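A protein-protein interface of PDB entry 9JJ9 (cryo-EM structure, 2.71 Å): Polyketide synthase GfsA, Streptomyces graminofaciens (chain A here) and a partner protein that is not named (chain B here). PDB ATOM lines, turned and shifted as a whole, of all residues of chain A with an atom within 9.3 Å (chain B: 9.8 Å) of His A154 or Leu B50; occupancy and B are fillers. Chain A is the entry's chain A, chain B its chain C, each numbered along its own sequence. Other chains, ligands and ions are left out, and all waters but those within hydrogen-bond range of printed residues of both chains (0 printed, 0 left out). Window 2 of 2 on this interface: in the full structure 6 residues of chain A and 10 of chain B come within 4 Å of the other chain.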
ATOM      1  N   SER A  92      35.163 -24.079 -23.809  1.00  0.00           N
ATOM      2  CA  SER A  92      34.537 -23.609 -22.585  1.00  0.00           C
ATOM      3  C   SER A  92      34.370 -24.760 -21.593  1.00  0.00           C
ATOM      4  O   SER A  92      34.188 -25.913 -21.991  1.00  0.00           O
ATOM      5  CB  SER A  92      33.177 -22.983 -22.887  1.00  0.00           C
ATOM      6  OG  SER A  92      33.321 -21.800 -23.654  1.00  0.00           O
ATOM      7  N   ARG A  94      31.862 -25.508 -19.733  1.00  0.00           N
ATOM      8  CA  ARG A  94      30.552 -26.135 -19.880  1.00  0.00           C
ATOM      9  C   ARG A  94      30.555 -27.160 -21.008  1.00  0.00           C
ATOM     10  O   ARG A  94      29.994 -28.252 -20.866  1.00  0.00           O
ATOM     11  CB  ARG A  94      29.483 -25.069 -20.124  1.00  0.00           C
ATOM     12  CG  ARG A  94      28.071 -25.521 -19.789  1.00  0.00           C
ATOM     13  CD  ARG A  94      27.055 -24.434 -20.097  1.00  0.00           C
ATOM     14  NE  ARG A  94      26.669 -24.429 -21.503  1.00  0.00           N
ATOM     15  CZ  ARG A  94      25.783 -23.598 -22.035  1.00  0.00           C
ATOM     16  NH1 ARG A  94      25.166 -22.685 -21.302  1.00  0.00           N
ATOM     17  NH2 ARG A  94      25.509 -23.685 -23.333  1.00  0.00           N
ATOM     18  N   GLU A  95      31.179 -26.822 -22.139  1.00  0.00           N
ATOM     19  CA  GLU A  95      31.290 -27.777 -23.237  1.00  0.00           C
ATOM     20  C   GLU A  95      32.181 -28.953 -22.856  1.00  0.00           C
ATOM     21  O   GLU A  95      31.890 -30.101 -23.213  1.00  0.00           O
ATOM     22  CB  GLU A  95      31.824 -27.076 -24.487  1.00  0.00           C
ATOM     23  CG  GLU A  95      32.131 -28.009 -25.646  1.00  0.00           C
ATOM     24  CD  GLU A  95      32.724 -27.281 -26.837  1.00  0.00           C
ATOM     25  OE1 GLU A  95      33.305 -26.193 -26.643  1.00  0.00           O
ATOM     26  OE2 GLU A  95      32.607 -27.798 -27.970  1.00  0.00           O
ATOM     27  N   ALA A  98      30.424 -31.877 -20.751  1.00  0.00           N
ATOM     28  CA  ALA A  98      29.715 -32.872 -21.542  1.00  0.00           C
ATOM     29  C   ALA A  98      30.582 -33.485 -22.632  1.00  0.00           C
ATOM     30  O   ALA A  98      30.120 -34.385 -23.341  1.00  0.00           O
ATOM     31  CB  ALA A  98      28.460 -32.254 -22.168  1.00  0.00           C
ATOM     32  N   TYR A 144      25.744 -41.010 -19.592  1.00  0.00           N
ATOM     33  CA  TYR A 144      24.896 -39.823 -19.596  1.00  0.00           C
ATOM     34  C   TYR A 144      23.426 -40.199 -19.753  1.00  0.00           C
ATOM     35  O   TYR A 144      22.549 -39.556 -19.165  1.00  0.00           O
ATOM     36  CB  TYR A 144      25.367 -38.859 -20.697  1.00  0.00           C
ATOM     37  CG  TYR A 144      24.384 -37.784 -21.143  1.00  0.00           C
ATOM     38  CD1 TYR A 144      23.270 -38.088 -21.921  1.00  0.00           C
ATOM     39  CD2 TYR A 144      24.577 -36.457 -20.777  1.00  0.00           C
ATOM     40  CE1 TYR A 144      22.386 -37.103 -22.320  1.00  0.00           C
ATOM     41  CE2 TYR A 144      23.698 -35.468 -21.171  1.00  0.00           C
ATOM     42  CZ  TYR A 144      22.605 -35.795 -21.942  1.00  0.00           C
ATOM     43  OH  TYR A 144      21.727 -34.814 -22.337  1.00  0.00           O
ATOM     44  N   VAL A 152      18.803 -31.703 -20.632  1.00  0.00           N
ATOM     45  CA  VAL A 152      19.484 -31.988 -21.888  1.00  0.00           C
ATOM     46  C   VAL A 152      19.829 -30.688 -22.606  1.00  0.00           C
ATOM     47  O   VAL A 152      18.944 -29.920 -22.982  1.00  0.00           O
ATOM     48  CB  VAL A 152      18.632 -32.897 -22.790  1.00  0.00           C
ATOM     49  CG1 VAL A 152      19.404 -33.271 -24.046  1.00  0.00           C
ATOM     50  CG2 VAL A 152      18.200 -34.142 -22.031  1.00  0.00           C
ATOM     51  N   ASP A 153      21.124 -30.448 -22.795  1.00  0.00           N
ATOM     52  CA  ASP A 153      21.610 -29.253 -23.463  1.00  0.00           C
ATOM     53  C   ASP A 153      21.981 -29.574 -24.909  1.00  0.00           C
ATOM     54  O   ASP A 153      21.820 -30.701 -25.388  1.00  0.00           O
ATOM     55  CB  ASP A 153      22.801 -28.664 -22.702  1.00  0.00           C
ATOM     56  CG  ASP A 153      23.935 -29.656 -22.539  1.00  0.00           C
ATOM     57  OD1 ASP A 153      23.656 -30.870 -22.444  1.00  0.00           O
ATOM     58  OD2 ASP A 153      25.106 -29.223 -22.505  1.00  0.00           O
ATOM     59  N   HIS A 154      22.486 -28.564 -25.613  1.00  0.00           N
ATOM     60  CA  HIS A 154      22.874 -28.712 -27.009  1.00  0.00           C
ATOM     61  C   HIS A 154      24.264 -29.307 -27.185  1.00  0.00           C
ATOM     62  O   HIS A 154      24.625 -29.674 -28.309  1.00  0.00           O
ATOM     63  CB  HIS A 154      22.809 -27.356 -27.722  1.00  0.00           C
ATOM     64  CG  HIS A 154      23.944 -26.441 -27.386  1.00  0.00           C
ATOM     65  ND1 HIS A 154      25.102 -26.385 -28.132  1.00  0.00           N
ATOM     66  CD2 HIS A 154      24.100 -25.544 -26.382  1.00  0.00           C
ATOM     67  CE1 HIS A 154      25.921 -25.494 -27.603  1.00  0.00           C
ATOM     68  NE2 HIS A 154      25.337 -24.969 -26.541  1.00  0.00           N
ATOM     69  N   HIS A 155      25.050 -29.414 -26.112  1.00  0.00           N
ATOM     70  CA  HIS A 155      26.388 -29.980 -26.213  1.00  0.00           C
ATOM     71  C   HIS A 155      26.385 -31.502 -26.236  1.00  0.00           C
ATOM     72  O   HIS A 155      27.405 -32.105 -26.587  1.00  0.00           O
ATOM     73  CB  HIS A 155      27.257 -29.489 -25.053  1.00  0.00           C
ATOM     74  CG  HIS A 155      27.672 -28.056 -25.171  1.00  0.00           C
ATOM     75  ND1 HIS A 155      27.352 -27.109 -24.222  1.00  0.00           N
ATOM     76  CD2 HIS A 155      28.382 -27.408 -26.125  1.00  0.00           C
ATOM     77  CE1 HIS A 155      27.846 -25.939 -24.587  1.00  0.00           C
ATOM     78  NE2 HIS A 155      28.475 -26.094 -25.737  1.00  0.00           N
ATOM     79  N   ALA A 156      25.266 -32.134 -25.867  1.00  0.00           N
ATOM     80  CA  ALA A 156      25.210 -33.592 -25.841  1.00  0.00           C
ATOM     81  C   ALA A 156      25.374 -34.180 -27.237  1.00  0.00           C
ATOM     82  O   ALA A 156      26.079 -35.179 -27.418  1.00  0.00           O
ATOM     83  CB  ALA A 156      23.895 -34.055 -25.213  1.00  0.00           C
ATOM     84  N   MET A 157      24.724 -33.577 -28.236  1.00  0.00           N
ATOM     85  CA  MET A 157      24.832 -34.085 -29.599  1.00  0.00           C
ATOM     86  C   MET A 157      26.256 -33.968 -30.126  1.00  0.00           C
ATOM     87  O   MET A 157      26.757 -34.880 -30.794  1.00  0.00           O
ATOM     88  CB  MET A 157      23.859 -33.341 -30.515  1.00  0.00           C
ATOM     89  CG  MET A 157      23.183 -34.223 -31.552  1.00  0.00           C
ATOM     90  SD  MET A 157      22.685 -33.308 -33.023  1.00  0.00           S
ATOM     91  CE  MET A 157      24.281 -32.844 -33.690  1.00  0.00           C
ATOM     92  N   THR A 158      26.925 -32.851 -29.837  1.00  0.00           N
ATOM     93  CA  THR A 158      28.279 -32.640 -30.336  1.00  0.00           C
ATOM     94  C   THR A 158      29.311 -33.472 -29.585  1.00  0.00           C
ATOM     95  O   THR A 158      30.318 -33.878 -30.175  1.00  0.00           O
ATOM     96  CB  THR A 158      28.647 -31.157 -30.251  1.00  0.00           C
ATOM     97  OG1 THR A 158      27.482 -30.360 -30.498  1.00  0.00           O
ATOM     98  CG2 THR A 158      29.716 -30.815 -31.279  1.00  0.00           C
ATOM     99  N   GLY A 159      29.087 -33.737 -28.301  1.00  0.00           N
ATOM    100  CA  GLY A 159      30.054 -34.429 -27.478  1.00  0.00           C
ATOM    101  C   GLY A 159      29.861 -35.918 -27.309  1.00  0.00           C
ATOM    102  O   GLY A 159      30.686 -36.561 -26.653  1.00  0.00           O
ATOM    103  N   LEU A 160      28.800 -36.497 -27.877  1.00  0.00           N
ATOM    104  CA  LEU A 160      28.519 -37.921 -27.719  1.00  0.00           C
ATOM    105  C   LEU A 160      28.463 -38.654 -29.054  1.00  0.00           C
ATOM    106  O   LEU A 160      27.771 -39.672 -29.168  1.00  0.00           O
ATOM    107  CB  LEU A 160      27.215 -38.126 -26.943  1.00  0.00           C
ATOM    108  CG  LEU A 160      27.218 -37.656 -25.487  1.00  0.00           C
ATOM    109  CD1 LEU A 160      25.954 -38.107 -24.771  1.00  0.00           C
ATOM    110  CD2 LEU A 160      28.456 -38.165 -24.762  1.00  0.00           C
ATOM    111  N   HIS A 161      29.173 -38.166 -30.067  1.00  0.00           N
ATOM    112  CA  HIS A 161      29.229 -38.810 -31.371  1.00  0.00           C
ATOM    113  C   HIS A 161      30.670 -39.161 -31.717  1.00  0.00           C
ATOM    114  O   HIS A 161      31.603 -38.450 -31.330  1.00  0.00           O
ATOM    115  CB  HIS A 161      28.625 -37.915 -32.456  1.00  0.00           C
ATOM    116  CG  HIS A 161      27.149 -38.091 -32.631  1.00  0.00           C
ATOM    117  ND1 HIS A 161      26.224 -37.264 -32.028  1.00  0.00           N
ATOM    118  CD2 HIS A 161      26.437 -39.000 -33.338  1.00  0.00           C
ATOM    119  CE1 HIS A 161      25.007 -37.655 -32.358  1.00  0.00           C
ATOM    120  NE2 HIS A 161      25.108 -38.706 -33.152  1.00  0.00           N
ATOM    121  N   ARG A 168      37.149 -32.848 -34.409  1.00  0.00           N
ATOM    122  CA  ARG A 168      37.736 -31.831 -33.546  1.00  0.00           C
ATOM    123  C   ARG A 168      39.208 -31.619 -33.871  1.00  0.00           C
ATOM    124  O   ARG A 168      39.698 -30.484 -33.854  1.00  0.00           O
ATOM    125  CB  ARG A 168      37.553 -32.222 -32.080  1.00  0.00           C
ATOM    126  CG  ARG A 168      36.143 -31.994 -31.560  1.00  0.00           C
ATOM    127  CD  ARG A 168      36.092 -32.039 -30.044  1.00  0.00           C
ATOM    128  NE  ARG A 168      34.722 -32.050 -29.547  1.00  0.00           N
ATOM    129  CZ  ARG A 168      33.975 -30.967 -29.380  1.00  0.00           C
ATOM    130  NH1 ARG A 168      34.437 -29.760 -29.660  1.00  0.00           N
ATOM    131  NH2 ARG A 168      32.734 -31.099 -28.921  1.00  0.00           N
ATOM    132  N   VAL B  27      27.100 -17.927 -17.808  1.00  0.00           N
ATOM    133  CA  VAL B  27      26.669 -18.927 -18.775  1.00  0.00           C
ATOM    134  C   VAL B  27      27.861 -19.614 -19.427  1.00  0.00           C
ATOM    135  O   VAL B  27      27.717 -20.709 -19.983  1.00  0.00           O
ATOM    136  CB  VAL B  27      25.745 -18.284 -19.834  1.00  0.00           C
ATOM    137  CG1 VAL B  27      26.561 -17.534 -20.879  1.00  0.00           C
ATOM    138  CG2 VAL B  27      24.863 -19.339 -20.487  1.00  0.00           C
ATOM    139  N   GLY B  46      35.215 -18.977 -26.288  1.00  0.00           N
ATOM    140  CA  GLY B  46      34.166 -19.929 -26.599  1.00  0.00           C
ATOM    141  C   GLY B  46      32.790 -19.308 -26.723  1.00  0.00           C
ATOM    142  O   GLY B  46      32.129 -19.042 -25.716  1.00  0.00           O
ATOM    143  N   PHE B  47      32.345 -19.084 -27.960  1.00  0.00           N
ATOM    144  CA  PHE B  47      31.029 -18.498 -28.206  1.00  0.00           C
ATOM    145  C   PHE B  47      30.578 -18.910 -29.601  1.00  0.00           C
ATOM    146  O   PHE B  47      31.135 -18.436 -30.594  1.00  0.00           O
ATOM    147  CB  PHE B  47      31.074 -16.980 -28.072  1.00  0.00           C
ATOM    148  CG  PHE B  47      30.451 -16.460 -26.808  1.00  0.00           C
ATOM    149  CD1 PHE B  47      29.076 -16.327 -26.703  1.00  0.00           C
ATOM    150  CD2 PHE B  47      31.237 -16.100 -25.727  1.00  0.00           C
ATOM    151  CE1 PHE B  47      28.497 -15.847 -25.544  1.00  0.00           C
ATOM    152  CE2 PHE B  47      30.664 -15.619 -24.564  1.00  0.00           C
ATOM    153  CZ  PHE B  47      29.292 -15.493 -24.474  1.00  0.00           C
ATOM    154  N   ASP B  48      29.580 -19.785 -29.671  1.00  0.00           N
ATOM    155  CA  ASP B  48      28.969 -20.165 -30.932  1.00  0.00           C
ATOM    156  C   ASP B  48      27.721 -19.314 -31.163  1.00  0.00           C
ATOM    157  O   ASP B  48      27.461 -18.345 -30.443  1.00  0.00           O
ATOM    158  CB  ASP B  48      28.662 -21.668 -30.944  1.00  0.00           C
ATOM    159  CG  ASP B  48      27.911 -22.126 -29.710  1.00  0.00           C
ATOM    160  OD1 ASP B  48      27.382 -21.267 -28.976  1.00  0.00           O
ATOM    161  OD2 ASP B  48      27.849 -23.350 -29.473  1.00  0.00           O
ATOM    162  N   SER B  49      26.940 -19.671 -32.184  1.00  0.00           N
ATOM    163  CA  SER B  49      25.741 -18.902 -32.502  1.00  0.00           C
ATOM    164  C   SER B  49      24.723 -18.963 -31.369  1.00  0.00           C
ATOM    165  O   SER B  49      24.087 -17.954 -31.043  1.00  0.00           O
ATOM    166  CB  SER B  49      25.123 -19.408 -33.805  1.00  0.00           C
ATOM    167  OG  SER B  49      26.126 -19.802 -34.725  1.00  0.00           O
ATOM    168  N   LEU B  50      24.553 -20.138 -30.759  1.00  0.00           N
ATOM    169  CA  LEU B  50      23.544 -20.298 -29.714  1.00  0.00           C
ATOM    170  C   LEU B  50      23.861 -19.427 -28.503  1.00  0.00           C
ATOM    171  O   LEU B  50      22.989 -18.713 -27.992  1.00  0.00           O
ATOM    172  CB  LEU B  50      23.432 -21.767 -29.303  1.00  0.00           C
ATOM    173  CG  LEU B  50      22.782 -22.769 -30.265  1.00  0.00           C
ATOM    174  CD1 LEU B  50      23.681 -23.098 -31.452  1.00  0.00           C
ATOM    175  CD2 LEU B  50      22.384 -24.039 -29.526  1.00  0.00           C
ATOM    176  N   MET B  51      25.109 -19.471 -28.029  1.00  0.00           N
ATOM    177  CA  MET B  51      25.487 -18.655 -26.880  1.00  0.00           C
ATOM    178  C   MET B  51      25.445 -17.170 -27.219  1.00  0.00           C
ATOM    179  O   MET B  51      25.084 -16.347 -26.372  1.00  0.00           O
ATOM    180  CB  MET B  51      26.873 -19.054 -26.372  1.00  0.00           C
ATOM    181  CG  MET B  51      26.996 -20.515 -25.971  1.00  0.00           C
ATOM    182  SD  MET B  51      28.669 -20.949 -25.454  1.00  0.00           S
ATOM    183  CE  MET B  51      28.764 -22.650 -26.005  1.00  0.00           C
ATOM    184  N   SER B  52      25.815 -16.809 -28.449  1.00  0.00           N
ATOM    185  CA  SER B  52      25.735 -15.410 -28.859  1.00  0.00           C
ATOM    186  C   SER B  52      24.296 -14.909 -28.827  1.00  0.00           C
ATOM    187  O   SER B  52      24.022 -13.817 -28.314  1.00  0.00           O
ATOM    188  CB  SER B  52      26.333 -15.237 -30.255  1.00  0.00           C
ATOM    189  OG  SER B  52      25.689 -14.190 -30.960  1.00  0.00           O
ATOM    190  N   VAL B  53      23.361 -15.703 -29.357  1.00  0.00           N
ATOM    191  CA  VAL B  53      21.953 -15.314 -29.338  1.00  0.00           C
ATOM    192  C   VAL B  53      21.440 -15.235 -27.905  1.00  0.00           C
ATOM    193  O   VAL B  53      20.711 -14.304 -27.540  1.00  0.00           O
ATOM    194  CB  VAL B  53      21.119 -16.289 -30.190  1.00  0.00           C
ATOM    195  CG1 VAL B  53      19.632 -16.040 -29.988  1.00  0.00           C
ATOM    196  CG2 VAL B  53      21.485 -16.153 -31.660  1.00  0.00           C
ATOM    197  N   GLU B  54      21.814 -16.209 -27.071  1.00  0.00           N
ATOM    198  CA  GLU B  54      21.370 -16.202 -25.680  1.00  0.00           C
ATOM    199  C   GLU B  54      21.877 -14.967 -24.944  1.00  0.00           C
ATOM    200  O   GLU B  54      21.126 -14.331 -24.197  1.00  0.00           O
ATOM    201  CB  GLU B  54      21.834 -17.477 -24.975  1.00  0.00           C
ATOM    202  CG  GLU B  54      21.482 -17.535 -23.498  1.00  0.00           C
ATOM    203  CD  GLU B  54      20.840 -18.851 -23.103  1.00  0.00           C
ATOM    204  OE1 GLU B  54      20.138 -19.447 -23.947  1.00  0.00           O
ATOM    205  OE2 GLU B  54      21.037 -19.288 -21.951  1.00  0.00           O
ATOM    206  N   LEU B  55      23.147 -14.607 -25.150  1.00  0.00           N
ATOM    207  CA  LEU B  55      23.697 -13.423 -24.500  1.00  0.00           C
ATOM    208  C   LEU B  55      23.068 -12.144 -25.036  1.00  0.00           C
ATOM    209  O   LEU B  55      22.874 -11.188 -24.277  1.00  0.00           O
ATOM    210  CB  LEU B  55      25.215 -13.385 -24.673  1.00  0.00           C
ATOM    211  CG  LEU B  55      25.979 -12.508 -23.679  1.00  0.00           C
ATOM    212  CD1 LEU B  55      26.160 -13.235 -22.355  1.00  0.00           C
ATOM    213  CD2 LEU B  55      27.324 -12.089 -24.250  1.00  0.00           C
ATOM    214  N   ARG B  56      22.749 -12.103 -26.333  1.00  0.00           N
ATOM    215  CA  ARG B  56      22.042 -10.949 -26.877  1.00  0.00           C
ATOM    216  C   ARG B  56      20.654 -10.807 -26.269  1.00  0.00           C
ATOM    217  O   ARG B  56      20.203  -9.686 -26.010  1.00  0.00           O
ATOM    218  CB  ARG B  56      21.950 -11.053 -28.399  1.00  0.00           C
ATOM    219  CG  ARG B  56      23.243 -10.712 -29.124  1.00  0.00           C
ATOM    220  CD  ARG B  56      23.253 -11.270 -30.538  1.00  0.00           C
ATOM    221  NE  ARG B  56      21.908 -11.519 -31.043  1.00  0.00           N
ATOM    222  CZ  ARG B  56      21.294 -10.764 -31.943  1.00  0.00           C
ATOM    223  NH1 ARG B  56      21.877  -9.696 -32.463  1.00  0.00           N
ATOM    224  NH2 ARG B  56      20.064 -11.088 -32.331  1.00  0.00           N
ATOM    225  N   ASP B  57      19.965 -11.923 -26.034  1.00  0.00           N
ATOM    226  CA  ASP B  57      18.650 -11.903 -25.409  1.00  0.00           C
ATOM    227  C   ASP B  57      18.713 -11.799 -23.890  1.00  0.00           C
ATOM    228  O   ASP B  57      17.673 -11.591 -23.256  1.00  0.00           O
ATOM    229  CB  ASP B  57      17.859 -13.156 -25.805  1.00  0.00           C
ATOM    230  CG  ASP B  57      17.794 -13.353 -27.306  1.00  0.00           C
ATOM    231  OD1 ASP B  57      17.825 -12.345 -28.042  1.00  0.00           O
ATOM    232  OD2 ASP B  57      17.712 -14.518 -27.751  1.00  0.00           O
ATOM    233  N   ARG B  58      19.896 -11.933 -23.293  1.00  0.00           N
ATOM    234  CA  ARG B  58      20.051 -11.823 -21.848  1.00  0.00           C
ATOM    235  C   ARG B  58      20.248 -10.391 -21.374  1.00  0.00           C
ATOM    236  O   ARG B  58      20.265 -10.155 -20.160  1.00  0.00           O
ATOM    237  CB  ARG B  58      21.233 -12.678 -21.374  1.00  0.00           C
ATOM    238  CG  ARG B  58      20.878 -14.123 -21.038  1.00  0.00           C
ATOM    239  CD  ARG B  58      20.603 -14.310 -19.552  1.00  0.00           C
ATOM    240  NE  ARG B  58      19.531 -13.449 -19.066  1.00  0.00           N
ATOM    241  CZ  ARG B  58      18.238 -13.688 -19.241  1.00  0.00           C
ATOM    242  NH1 ARG B  58      17.816 -14.764 -19.886  1.00  0.00           N
ATOM    243  NH2 ARG B  58      17.347 -12.828 -18.757  1.00  0.00           N
ATOM    244  N   LEU B  72      26.878  -7.191 -30.805  1.00  0.00           N
ATOM    245  CA  LEU B  72      27.735  -8.271 -30.331  1.00  0.00           C
ATOM    246  C   LEU B  72      28.667  -8.755 -31.437  1.00  0.00           C
ATOM    247  O   LEU B  72      29.823  -9.100 -31.174  1.00  0.00           O
ATOM    248  CB  LEU B  72      26.890  -9.433 -29.806  1.00  0.00           C
ATOM    249  CG  LEU B  72      27.640 -10.511 -29.020  1.00  0.00           C
ATOM    250  CD1 LEU B  72      26.980 -10.743 -27.671  1.00  0.00           C
ATOM    251  CD2 LEU B  72      27.714 -11.803 -29.816  1.00  0.00           C
ATOM    252  N   TYR B  73      28.167  -8.787 -32.675  1.00  0.00           N
ATOM    253  CA  TYR B  73      28.992  -9.235 -33.793  1.00  0.00           C
ATOM    254  C   TYR B  73      30.163  -8.289 -34.033  1.00  0.00           C
ATOM    255  O   TYR B  73      31.283  -8.735 -34.303  1.00  0.00           O
ATOM    256  CB  TYR B  73      28.138  -9.369 -35.053  1.00  0.00           C
ATOM    257  CG  TYR B  73      26.906 -10.228 -34.866  1.00  0.00           C
ATOM    258  CD1 TYR B  73      27.002 -11.613 -34.825  1.00  0.00           C
ATOM    259  CD2 TYR B  73      25.649  -9.654 -34.727  1.00  0.00           C
ATOM    260  CE1 TYR B  73      25.881 -12.402 -34.653  1.00  0.00           C
ATOM    261  CE2 TYR B  73      24.522 -10.435 -34.553  1.00  0.00           C
ATOM    262  CZ  TYR B  73      24.644 -11.808 -34.517  1.00  0.00           C
ATOM    263  OH  TYR B  73      23.524 -12.590 -34.346  1.00  0.00           O
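NH1 of Arg A94 sits close to O of Val B27, at 3.5 Å.
The guanidinium group of Arg A94 is in hydrogen-bond range of a ring nitrogen (NE2) of His A154.
A ring nitrogen (NE2) of His A154 sits close to a ring nitrogen (NE2) of His A155, 3.4 Å away.
The side-chain carboxylate (OD1) of Asp B48 sits at hydrogen-bond distance from the backbone NH (N) of Met B51 (3.0 Å).
Among the printed residues, merely in contact across the chains: Ser A92 with Gly B46, His A154 with Asp B48, His A154 with Leu B50 and His A155 with Met B51.
Of the printed residues of chain B, Ser A92 touches Gly B46 (3.6 Å).
Printed residues of chain B within 4 Å of Arg A94: Val B27 (3.5 Å).
No residue of chain B comes within 4 Å of Asp A153.
Of chain B, only Asp B48 (3.4 Å) and Leu B50 (3.6 Å) come within 4 Å of His A154.
His A155 touches just one residue of chain B: Met B51.
Leu A160 touches none of the printed residues of chain B.
Printed residues of chain A within 4 Å of Gly B46: Ser A92.
Leu B50 touches just one residue of chain A: His A154 (3.6 Å).
Printed residues of chain A within 4 Å of Met B51: His A155 (3.5 Å).
Tyr B73 touches none of the printed residues of chain A.
The nearest residue of chain B that does not touch His A154 is Met B51 (4.2 Å).
The nearest printed residue of chain B that does not touch Ser A92 is Met B51 (5.1 Å).
Hydrophobic or aromatic side chains of chain B that line the printed part of chain A: Val B27, Leu B50 and Met B51.
Of the 16 printed residues of chain A, 4 touch a printed residue of chain B.
Hydrophobic or aromatic side chains of chain A that line the printed part of chain B: His A154 and His A155.
Among the printed residues, no Asp or Glu carboxylate lies within 4 Å of a Lys or Arg side-chain nitrogen of the other chain.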
